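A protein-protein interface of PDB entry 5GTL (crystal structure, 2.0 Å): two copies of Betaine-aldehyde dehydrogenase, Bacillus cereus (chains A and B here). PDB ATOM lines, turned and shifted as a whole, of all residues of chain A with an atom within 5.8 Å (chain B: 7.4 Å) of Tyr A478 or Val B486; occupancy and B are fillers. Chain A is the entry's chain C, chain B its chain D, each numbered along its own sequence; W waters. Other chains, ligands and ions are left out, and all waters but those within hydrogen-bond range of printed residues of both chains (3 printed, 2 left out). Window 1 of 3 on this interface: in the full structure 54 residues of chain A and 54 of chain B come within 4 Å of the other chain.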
ATOM      1  N   ALA A 446      23.965  10.724   4.869  1.00  0.00           N
ATOM      2  CA  ALA A 446      24.043   9.332   4.425  1.00  0.00           C
ATOM      3  C   ALA A 446      24.342   9.248   2.937  1.00  0.00           C
ATOM      4  O   ALA A 446      23.883  10.086   2.144  1.00  0.00           O
ATOM      5  CB  ALA A 446      22.706   8.628   4.736  1.00  0.00           C
ATOM      6  N   GLY A 447      25.054   8.194   2.564  1.00  0.00           N
ATOM      7  CA  GLY A 447      25.442   7.949   1.182  1.00  0.00           C
ATOM      8  C   GLY A 447      24.318   7.735   0.227  1.00  0.00           C
ATOM      9  O   GLY A 447      24.489   8.024  -0.944  1.00  0.00           O
ATOM     10  N   THR A 448      23.196   7.154   0.704  1.00  0.00           N
ATOM     11  CA  THR A 448      22.086   6.873  -0.146  1.00  0.00           C
ATOM     12  C   THR A 448      20.839   7.263   0.631  1.00  0.00           C
ATOM     13  O   THR A 448      20.774   6.971   1.795  1.00  0.00           O
ATOM     14  CB  THR A 448      21.975   5.346  -0.500  1.00  0.00           C
ATOM     15  OG1 THR A 448      23.080   4.925  -1.324  1.00  0.00           O
ATOM     16  CG2 THR A 448      20.672   5.094  -1.226  1.00  0.00           C
ATOM     17  N   PRO A 462      25.783   4.645  -7.127  1.00  0.00           N
ATOM     18  CA  PRO A 462      26.750   4.368  -6.080  1.00  0.00           C
ATOM     19  C   PRO A 462      26.168   4.254  -4.708  1.00  0.00           C
ATOM     20  O   PRO A 462      25.167   4.847  -4.481  1.00  0.00           O
ATOM     21  CB  PRO A 462      27.638   5.590  -6.113  1.00  0.00           C
ATOM     22  CG  PRO A 462      26.745   6.664  -6.513  1.00  0.00           C
ATOM     23  CD  PRO A 462      25.815   6.056  -7.508  1.00  0.00           C
ATOM     24  N   GLY A 464      27.460   3.813  -0.335  1.00  0.00           N
ATOM     25  CA  GLY A 464      28.456   3.789   0.698  1.00  0.00           C
ATOM     26  C   GLY A 464      28.234   4.794   1.806  1.00  0.00           C
ATOM     27  O   GLY A 464      27.348   5.579   1.753  1.00  0.00           O
ATOM     28  N   TYR A 466      28.939   7.780   4.897  1.00  0.00           N
ATOM     29  CA  TYR A 466      29.469   9.001   5.405  1.00  0.00           C
ATOM     30  C   TYR A 466      29.999   8.534   6.771  1.00  0.00           C
ATOM     31  O   TYR A 466      29.748   7.444   7.208  1.00  0.00           O
ATOM     32  CB  TYR A 466      28.393  10.015   5.692  1.00  0.00           C
ATOM     33  CG  TYR A 466      27.884  10.860   4.545  1.00  0.00           C
ATOM     34  CD1 TYR A 466      27.485  10.312   3.362  1.00  0.00           C
ATOM     35  CD2 TYR A 466      27.789  12.216   4.680  1.00  0.00           C
ATOM     36  CE1 TYR A 466      26.998  11.105   2.351  1.00  0.00           C
ATOM     37  CE2 TYR A 466      27.315  13.011   3.683  1.00  0.00           C
ATOM     38  CZ  TYR A 466      26.937  12.462   2.516  1.00  0.00           C
ATOM     39  OH  TYR A 466      26.456  13.269   1.553  1.00  0.00           O
ATOM     40  N   ARG A 473      32.964   4.772  -2.423  1.00  0.00           N
ATOM     41  CA  ARG A 473      31.713   4.291  -2.867  1.00  0.00           C
ATOM     42  C   ARG A 473      31.785   3.035  -3.681  1.00  0.00           C
ATOM     43  O   ARG A 473      32.746   2.809  -4.358  1.00  0.00           O
ATOM     44  CB  ARG A 473      31.059   5.379  -3.697  1.00  0.00           C
ATOM     45  CG  ARG A 473      30.735   6.603  -2.901  1.00  0.00           C
ATOM     46  CD  ARG A 473      29.533   6.366  -2.049  1.00  0.00           C
ATOM     47  NE  ARG A 473      29.138   7.521  -1.299  1.00  0.00           N
ATOM     48  CZ  ARG A 473      29.592   7.861  -0.120  1.00  0.00           C
ATOM     49  NH1 ARG A 473      30.471   7.136   0.492  1.00  0.00           N
ATOM     50  NH2 ARG A 473      29.124   8.915   0.454  1.00  0.00           N
ATOM     51  N   GLU A 474      30.751   2.217  -3.587  1.00  0.00           N
ATOM     52  CA  GLU A 474      30.686   1.071  -4.472  1.00  0.00           C
ATOM     53  C   GLU A 474      29.600   1.294  -5.493  1.00  0.00           C
ATOM     54  O   GLU A 474      28.714   2.108  -5.260  1.00  0.00           O
ATOM     55  CB  GLU A 474      30.622  -0.232  -3.688  1.00  0.00           C
ATOM     56  CG  GLU A 474      32.055  -0.631  -3.298  1.00  0.00           C
ATOM     57  CD  GLU A 474      32.160  -1.759  -2.290  1.00  0.00           C
ATOM     58  OE1 GLU A 474      31.282  -1.902  -1.391  1.00  0.00           O
ATOM     59  OE2 GLU A 474      33.180  -2.478  -2.391  1.00  0.00           O
ATOM     60  N   LEU A 475      29.694   0.600  -6.635  1.00  0.00           N
ATOM     61  CA  LEU A 475      28.747   0.776  -7.771  1.00  0.00           C
ATOM     62  C   LEU A 475      28.789   2.081  -8.475  1.00  0.00           C
ATOM     63  O   LEU A 475      29.527   2.982  -8.104  1.00  0.00           O
ATOM     64  CB  LEU A 475      27.285   0.459  -7.321  1.00  0.00           C
ATOM     65  CG  LEU A 475      27.097  -0.942  -6.798  1.00  0.00           C
ATOM     66  CD1 LEU A 475      25.602  -1.168  -6.410  1.00  0.00           C
ATOM     67  CD2 LEU A 475      27.556  -1.966  -7.812  1.00  0.00           C
ATOM     68  N   GLY A 476      28.106   2.162  -9.620  1.00  0.00           N
ATOM     69  CA  GLY A 476      28.170   3.322 -10.412  1.00  0.00           C
ATOM     70  C   GLY A 476      29.533   3.506 -11.087  1.00  0.00           C
ATOM     71  O   GLY A 476      30.426   2.669 -10.940  1.00  0.00           O
ATOM     72  N   SER A 477      29.666   4.599 -11.839  1.00  0.00           N
ATOM     73  CA  SER A 477      30.993   5.053 -12.373  1.00  0.00           C
ATOM     74  C   SER A 477      31.993   5.228 -11.225  1.00  0.00           C
ATOM     75  O   SER A 477      33.169   4.979 -11.378  1.00  0.00           O
ATOM     76  CB  SER A 477      30.886   6.367 -13.107  1.00  0.00           C
ATOM     77  OG  SER A 477      30.366   7.350 -12.240  1.00  0.00           O
ATOM     78  N   TYR A 478      31.476   5.675 -10.101  1.00  0.00           N
ATOM     79  CA  TYR A 478      32.266   6.050  -8.944  1.00  0.00           C
ATOM     80  C   TYR A 478      33.188   4.931  -8.468  1.00  0.00           C
ATOM     81  O   TYR A 478      34.346   5.196  -8.161  1.00  0.00           O
ATOM     82  CB  TYR A 478      31.361   6.511  -7.795  1.00  0.00           C
ATOM     83  CG  TYR A 478      30.583   7.771  -8.098  1.00  0.00           C
ATOM     84  CD1 TYR A 478      31.133   9.055  -7.867  1.00  0.00           C
ATOM     85  CD2 TYR A 478      29.311   7.684  -8.620  1.00  0.00           C
ATOM     86  CE1 TYR A 478      30.393  10.182  -8.162  1.00  0.00           C
ATOM     87  CE2 TYR A 478      28.595   8.789  -8.926  1.00  0.00           C
ATOM     88  CZ  TYR A 478      29.100  10.036  -8.674  1.00  0.00           C
ATOM     89  OH  TYR A 478      28.303  11.111  -9.025  1.00  0.00           O
ATOM     90  N   ALA A 479      32.697   3.694  -8.462  1.00  0.00           N
ATOM     91  CA  ALA A 479      33.556   2.596  -7.961  1.00  0.00           C
ATOM     92  C   ALA A 479      34.836   2.475  -8.740  1.00  0.00           C
ATOM     93  O   ALA A 479      35.838   1.994  -8.238  1.00  0.00           O
ATOM     94  CB  ALA A 479      32.801   1.269  -8.005  1.00  0.00           C
ATOM     95  N   LEU A 480      34.789   2.856  -9.983  1.00  0.00           N
ATOM     96  CA  LEU A 480      35.944   2.725 -10.849  1.00  0.00           C
ATOM     97  C   LEU A 480      37.120   3.525 -10.377  1.00  0.00           C
ATOM     98  O   LEU A 480      38.263   3.077 -10.543  1.00  0.00           O
ATOM     99  CB  LEU A 480      35.624   3.144 -12.317  1.00  0.00           C
ATOM    100  CG  LEU A 480      34.521   2.430 -13.032  1.00  0.00           C
ATOM    101  CD1 LEU A 480      34.034   3.207 -14.275  1.00  0.00           C
ATOM    102  CD2 LEU A 480      34.924   1.032 -13.400  1.00  0.00           C
ATOM    103  N   ASP A 481      36.880   4.703  -9.808  1.00  0.00           N
ATOM    104  CA  ASP A 481      37.991   5.561  -9.322  1.00  0.00           C
ATOM    105  C   ASP A 481      38.774   4.861  -8.178  1.00  0.00           C
ATOM    106  O   ASP A 481      39.951   5.107  -7.983  1.00  0.00           O
ATOM    107  CB  ASP A 481      37.511   6.891  -8.774  1.00  0.00           C
ATOM    108  CG  ASP A 481      36.737   7.694  -9.793  1.00  0.00           C
ATOM    109  OD1 ASP A 481      36.846   7.406 -10.962  1.00  0.00           O
ATOM    110  OD2 ASP A 481      35.986   8.598  -9.401  1.00  0.00           O
ATOM    111  N   ASN A 482      38.158   3.948  -7.492  1.00  0.00           N
ATOM    112  CA  ASN A 482      38.849   3.219  -6.448  1.00  0.00           C
ATOM    113  C   ASN A 482      39.905   2.288  -7.011  1.00  0.00           C
ATOM    114  O   ASN A 482      40.809   1.931  -6.331  1.00  0.00           O
ATOM    115  CB  ASN A 482      37.869   2.370  -5.662  1.00  0.00           C
ATOM    116  CG  ASN A 482      36.872   3.184  -4.899  1.00  0.00           C
ATOM    117  OD1 ASN A 482      35.752   2.822  -4.800  1.00  0.00           O
ATOM    118  ND2 ASN A 482      37.294   4.267  -4.354  1.00  0.00           N
ATOM    119  N   ILE B 139      29.482  19.126 -10.572  1.00  0.00           N
ATOM    120  CA  ILE B 139      28.260  18.432 -10.900  1.00  0.00           C
ATOM    121  C   ILE B 139      28.152  16.982 -10.505  1.00  0.00           C
ATOM    122  O   ILE B 139      29.093  16.265 -10.510  1.00  0.00           O
ATOM    123  CB  ILE B 139      27.878  18.554 -12.413  1.00  0.00           C
ATOM    124  CG1 ILE B 139      28.964  17.968 -13.313  1.00  0.00           C
ATOM    125  CG2 ILE B 139      27.591  19.982 -12.807  1.00  0.00           C
ATOM    126  CD1 ILE B 139      28.542  17.736 -14.743  1.00  0.00           C
ATOM    127  N   GLY B 140      26.934  16.600 -10.162  1.00  0.00           N
ATOM    128  CA  GLY B 140      26.579  15.249  -9.854  1.00  0.00           C
ATOM    129  C   GLY B 140      25.986  14.672 -11.130  1.00  0.00           C
ATOM    130  O   GLY B 140      26.078  15.274 -12.153  1.00  0.00           O
ATOM    131  N   GLN B 141      25.358  13.521 -11.027  1.00  0.00           N
ATOM    132  CA  GLN B 141      24.779  12.809 -12.131  1.00  0.00           C
ATOM    133  C   GLN B 141      23.273  12.554 -11.990  1.00  0.00           C
ATOM    134  O   GLN B 141      22.766  12.511 -10.916  1.00  0.00           O
ATOM    135  CB  GLN B 141      25.423  11.396 -12.203  1.00  0.00           C
ATOM    136  CG  GLN B 141      26.938  11.271 -12.154  1.00  0.00           C
ATOM    137  CD  GLN B 141      27.444   9.836 -12.333  1.00  0.00           C
ATOM    138  OE1 GLN B 141      26.717   8.891 -12.206  1.00  0.00           O
ATOM    139  NE2 GLN B 141      28.666   9.709 -12.668  1.00  0.00           N
ATOM    140  N   THR B 142      22.598  12.423 -13.119  1.00  0.00           N
ATOM    141  CA  THR B 142      21.232  11.934 -13.225  1.00  0.00           C
ATOM    142  C   THR B 142      21.530  10.571 -13.936  1.00  0.00           C
ATOM    143  O   THR B 142      22.317  10.480 -14.839  1.00  0.00           O
ATOM    144  CB  THR B 142      20.215  12.821 -13.948  1.00  0.00           C
ATOM    145  OG1 THR B 142      20.687  13.163 -15.232  1.00  0.00           O
ATOM    146  CG2 THR B 142      19.882  14.036 -13.119  1.00  0.00           C
ATOM    147  N   ILE B 143      20.928   9.516 -13.462  1.00  0.00           N
ATOM    148  CA  ILE B 143      21.222   8.198 -13.901  1.00  0.00           C
ATOM    149  C   ILE B 143      19.990   7.468 -14.362  1.00  0.00           C
ATOM    150  O   ILE B 143      19.089   7.224 -13.603  1.00  0.00           O
ATOM    151  CB  ILE B 143      21.943   7.431 -12.755  1.00  0.00           C
ATOM    152  CG1 ILE B 143      23.035   8.303 -12.112  1.00  0.00           C
ATOM    153  CG2 ILE B 143      22.450   6.094 -13.251  1.00  0.00           C
ATOM    154  CD1 ILE B 143      23.648   7.775 -10.846  1.00  0.00           C
ATOM    155  N   TYR B 152      19.621  10.426  -8.862  1.00  0.00           N
ATOM    156  CA  TYR B 152      20.609  11.511  -8.960  1.00  0.00           C
ATOM    157  C   TYR B 152      21.588  11.504  -7.831  1.00  0.00           C
ATOM    158  O   TYR B 152      21.219  11.064  -6.760  1.00  0.00           O
ATOM    159  CB  TYR B 152      19.939  12.885  -9.028  1.00  0.00           C
ATOM    160  CG  TYR B 152      19.213  13.444  -7.827  1.00  0.00           C
ATOM    161  CD1 TYR B 152      17.867  13.099  -7.544  1.00  0.00           C
ATOM    162  CD2 TYR B 152      19.797  14.362  -7.015  1.00  0.00           C
ATOM    163  CE1 TYR B 152      17.191  13.685  -6.490  1.00  0.00           C
ATOM    164  CE2 TYR B 152      19.125  14.925  -5.932  1.00  0.00           C
ATOM    165  CZ  TYR B 152      17.829  14.549  -5.676  1.00  0.00           C
ATOM    166  OH  TYR B 152      17.235  15.149  -4.632  1.00  0.00           O
ATOM    167  N   THR B 153      22.815  12.034  -8.080  1.00  0.00           N
ATOM    168  CA  THR B 153      23.789  12.160  -7.063  1.00  0.00           C
ATOM    169  C   THR B 153      24.097  13.631  -6.791  1.00  0.00           C
ATOM    170  O   THR B 153      23.853  14.486  -7.600  1.00  0.00           O
ATOM    171  CB  THR B 153      25.026  11.348  -7.373  1.00  0.00           C
ATOM    172  OG1 THR B 153      25.754  11.922  -8.468  1.00  0.00           O
ATOM    173  CG2 THR B 153      24.646   9.936  -7.699  1.00  0.00           C
ATOM    174  N   ARG B 154      24.501  13.900  -5.569  1.00  0.00           N
ATOM    175  CA  ARG B 154      24.913  15.204  -5.135  1.00  0.00           C
ATOM    176  C   ARG B 154      26.312  15.032  -4.657  1.00  0.00           C
ATOM    177  O   ARG B 154      26.592  14.103  -3.917  1.00  0.00           O
ATOM    178  CB  ARG B 154      24.083  15.675  -3.984  1.00  0.00           C
ATOM    179  CG  ARG B 154      22.803  16.328  -4.339  1.00  0.00           C
ATOM    180  CD  ARG B 154      21.899  16.416  -3.122  1.00  0.00           C
ATOM    181  NE  ARG B 154      22.468  17.106  -1.942  1.00  0.00           N
ATOM    182  CZ  ARG B 154      22.283  18.376  -1.612  1.00  0.00           C
ATOM    183  NH1 ARG B 154      21.560  19.207  -2.359  1.00  0.00           N
ATOM    184  NH2 ARG B 154      22.808  18.830  -0.492  1.00  0.00           N
ATOM    185  N   HIS B 155      27.204  15.934  -5.049  1.00  0.00           N
ATOM    186  CA  HIS B 155      28.532  15.922  -4.538  1.00  0.00           C
ATOM    187  C   HIS B 155      28.612  16.959  -3.416  1.00  0.00           C
ATOM    188  O   HIS B 155      28.931  18.084  -3.654  1.00  0.00           O
ATOM    189  CB  HIS B 155      29.545  16.214  -5.656  1.00  0.00           C
ATOM    190  CG  HIS B 155      29.624  15.136  -6.702  1.00  0.00           C
ATOM    191  ND1 HIS B 155      30.704  14.992  -7.549  1.00  0.00           N
ATOM    192  CD2 HIS B 155      28.778  14.112  -6.996  1.00  0.00           C
ATOM    193  CE1 HIS B 155      30.514  13.948  -8.331  1.00  0.00           C
ATOM    194  NE2 HIS B 155      29.343  13.398  -8.013  1.00  0.00           N
ATOM    195  N   GLU B 156      28.363  16.542  -2.191  1.00  0.00           N
ATOM    196  CA  GLU B 156      28.300  17.487  -1.055  1.00  0.00           C
ATOM    197  C   GLU B 156      29.679  17.775  -0.523  1.00  0.00           C
ATOM    198  O   GLU B 156      30.503  16.894  -0.545  1.00  0.00           O
ATOM    199  CB  GLU B 156      27.459  16.925   0.085  1.00  0.00           C
ATOM    200  CG  GLU B 156      26.037  16.599  -0.326  1.00  0.00           C
ATOM    201  CD  GLU B 156      25.142  16.120   0.813  1.00  0.00           C
ATOM    202  OE1 GLU B 156      25.650  15.726   1.882  1.00  0.00           O
ATOM    203  OE2 GLU B 156      23.924  16.055   0.618  1.00  0.00           O
ATOM    204  N   ASP B 481      37.383  15.743  -5.807  1.00  0.00           N
ATOM    205  CA  ASP B 481      36.748  14.513  -5.365  1.00  0.00           C
ATOM    206  C   ASP B 481      37.180  14.183  -3.905  1.00  0.00           C
ATOM    207  O   ASP B 481      36.431  13.512  -3.155  1.00  0.00           O
ATOM    208  CB  ASP B 481      37.202  13.357  -6.248  1.00  0.00           C
ATOM    209  CG  ASP B 481      36.678  13.452  -7.636  1.00  0.00           C
ATOM    210  OD1 ASP B 481      35.714  14.205  -7.845  1.00  0.00           O
ATOM    211  OD2 ASP B 481      37.261  12.788  -8.512  1.00  0.00           O
ATOM    212  N   THR B 484      34.632  15.926  -1.218  1.00  0.00           N
ATOM    213  CA  THR B 484      33.254  15.634  -1.416  1.00  0.00           C
ATOM    214  C   THR B 484      32.792  14.286  -0.892  1.00  0.00           C
ATOM    215  O   THR B 484      33.547  13.380  -0.825  1.00  0.00           O
ATOM    216  CB  THR B 484      33.020  15.789  -2.960  1.00  0.00           C
ATOM    217  OG1 THR B 484      32.768  17.158  -3.243  1.00  0.00           O
ATOM    218  CG2 THR B 484      31.932  15.041  -3.476  1.00  0.00           C
ATOM    219  N   GLU B 485      31.524  14.214  -0.550  1.00  0.00           N
ATOM    220  CA  GLU B 485      30.805  13.009  -0.175  1.00  0.00           C
ATOM    221  C   GLU B 485      29.697  12.874  -1.218  1.00  0.00           C
ATOM    222  O   GLU B 485      28.890  13.760  -1.382  1.00  0.00           O
ATOM    223  CB  GLU B 485      30.220  13.021   1.222  1.00  0.00           C
ATOM    224  CG  GLU B 485      31.223  12.784   2.325  1.00  0.00           C
ATOM    225  CD  GLU B 485      31.675  11.363   2.539  1.00  0.00           C
ATOM    226  OE1 GLU B 485      32.430  11.186   3.471  1.00  0.00           O
ATOM    227  OE2 GLU B 485      31.324  10.448   1.805  1.00  0.00           O
ATOM    228  N   VAL B 486      29.709  11.767  -1.933  1.00  0.00           N
ATOM    229  CA  VAL B 486      28.727  11.510  -2.949  1.00  0.00           C
ATOM    230  C   VAL B 486      27.499  10.945  -2.254  1.00  0.00           C
ATOM    231  O   VAL B 486      27.626  10.001  -1.460  1.00  0.00           O
ATOM    232  CB  VAL B 486      29.276  10.497  -3.936  1.00  0.00           C
ATOM    233  CG1 VAL B 486      28.202  10.070  -4.889  1.00  0.00           C
ATOM    234  CG2 VAL B 486      30.501  11.149  -4.645  1.00  0.00           C
ATOM    235  N   LYS B 487      26.340  11.526  -2.566  1.00  0.00           N
ATOM    236  CA  LYS B 487      25.044  11.074  -2.068  1.00  0.00           C
ATOM    237  C   LYS B 487      24.134  10.643  -3.224  1.00  0.00           C
ATOM    238  O   LYS B 487      23.915  11.424  -4.117  1.00  0.00           O
ATOM    239  CB  LYS B 487      24.382  12.175  -1.275  1.00  0.00           C
ATOM    240  CG  LYS B 487      22.978  11.844  -0.773  1.00  0.00           C
ATOM    241  CD  LYS B 487      22.340  13.048  -0.125  1.00  0.00           C
ATOM    242  CE  LYS B 487      22.801  13.242   1.326  1.00  0.00           C
ATOM    243  NZ  LYS B 487      22.184  14.537   1.830  1.00  0.00           N
ATOM    244  N   SER B 488      23.577   9.416  -3.188  1.00  0.00           N
ATOM    245  CA  SER B 488      22.718   8.938  -4.256  1.00  0.00           C
ATOM    246  C   SER B 488      21.313   9.030  -3.692  1.00  0.00           C
ATOM    247  O   SER B 488      21.036   8.397  -2.704  1.00  0.00           O
ATOM    248  CB  SER B 488      23.070   7.474  -4.693  1.00  0.00           C
ATOM    249  OG  SER B 488      21.949   6.786  -5.255  1.00  0.00           O
HETATM  250  O   HOH W   1      27.198   6.247 -11.269  1.00  0.00           O
HETATM  251  O   HOH W   2      22.606   4.270  -3.898  1.00  0.00           O
HETATM  252  O   HOH W   3      37.926  10.129  -7.464  1.00  0.00           O
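The backbone carbonyl oxygen (O) of Gly A447 is in hydrogen-bond range of the backbone NH (N) of Ser B488, at 2.8 Å.
OH of Tyr A466 sits at hydrogen-bond distance from OE1 of Glu B156 (2.6 Å).
The guanidinium group of Arg A473 is in salt-bridge range of the side-chain carboxylate of Glu B485 (3.0 Å).
The guanidinium group (NH2) of Arg A473 is in hydrogen-bond range of the backbone carbonyl oxygen (O) of Val B486 (2.7 Å).
OG of Ser A477 is in hydrogen-bond range of NE2 of Gln B141 (2.9 Å).
OH of Tyr A478 sits at hydrogen-bond distance from OG1 of Thr B153 (2.7 Å).
OH of Tyr A478 lies within hydrogen-bond range of NE2 of His B155, at 2.7 Å.
OD1 of Asn A482 sits close to O of Arg A473.
The backbone NH (N) of Thr B153 is in hydrogen-bond range of the backbone carbonyl oxygen (O) of Gln B141 (2.9 Å).
The side-chain carboxylate of Glu B156 is in salt-bridge range of the guanidinium group of Arg B154 (3.1 Å).
N of Lys B487 is in hydrogen-bond range of O of Arg B154, at 2.9 Å.
The backbone carbonyl oxygen (O) of Glu B156 lies within hydrogen-bond range of the backbone NH (N) of Glu B485, 2.9 Å away.
OE2 of Glu B156 is in salt-bridge range of NZ of Lys B487 (2.6 Å).
Ala A446 touches Lys B487.
O of Val B486 touches O of Gly A447, 3.7 Å away.
Gly A447 touches Lys B487.
CA of Thr A448 touches O of Ser B488, at 3.2 Å.
Pro A462 touches Ser B488 (O to CB, 3.4 Å).
Glu B485 touches Tyr A466.
Tyr A466 touches Lys B487.
Tyr A478 touches Gln B141.
Val B486 touches Tyr A478 (CG2 to CE1, 3.6 Å).
Of the printed residues of chain B, Arg A473 touches Glu B485 and Val B486.
Ser A477 touches just one residue of chain B: Gln B141 (2.9 Å).
Of chain B, only Gln B141, Thr B153, His B155 and Val B486 come within 4 Å of Tyr A478.
Asp A481 touches none of the printed residues of chain B.
Of the printed residues of chain A, His B155 touches Tyr A478 (2.7 Å).
Of the printed residues of chain A, Val B486 touches Gly A447, Arg A473 and Tyr A478.
The nearest residue of chain B that does not touch Tyr A478 is Gly B140 (4.6 Å).
The nearest printed residue of chain A that does not touch Val B486 is Tyr A466 (4.02 Å).
Hydrophobic or aromatic side chains of chain A that line the printed part of chain B: Tyr A466 and Tyr A478.
Of the 16 printed residues of chain B, 8 touch a printed residue of chain A.
Hydrophobic or aromatic side chains of chain B within 4 Å of the printed part of chain A: His B155 and Val B486.
Position printed for both chains: 481.
Water W2 lies within hydrogen-bond range of the backbone carbonyl oxygen of Pro A462 (2.7 Å), the side-chain hydroxyl of Thr A448 (2.7 Å) and the side-chain hydroxyl of Ser B488 (2.9 Å).
Water W1 bridges the side-chain amide oxygen (OE1) of Gln B141 (2.8 Å) and the backbone NH (N) of Ser A477 (3.0 Å).
Water W3 bridges OD2 of Asp B481 and OD2 of Asp A481.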
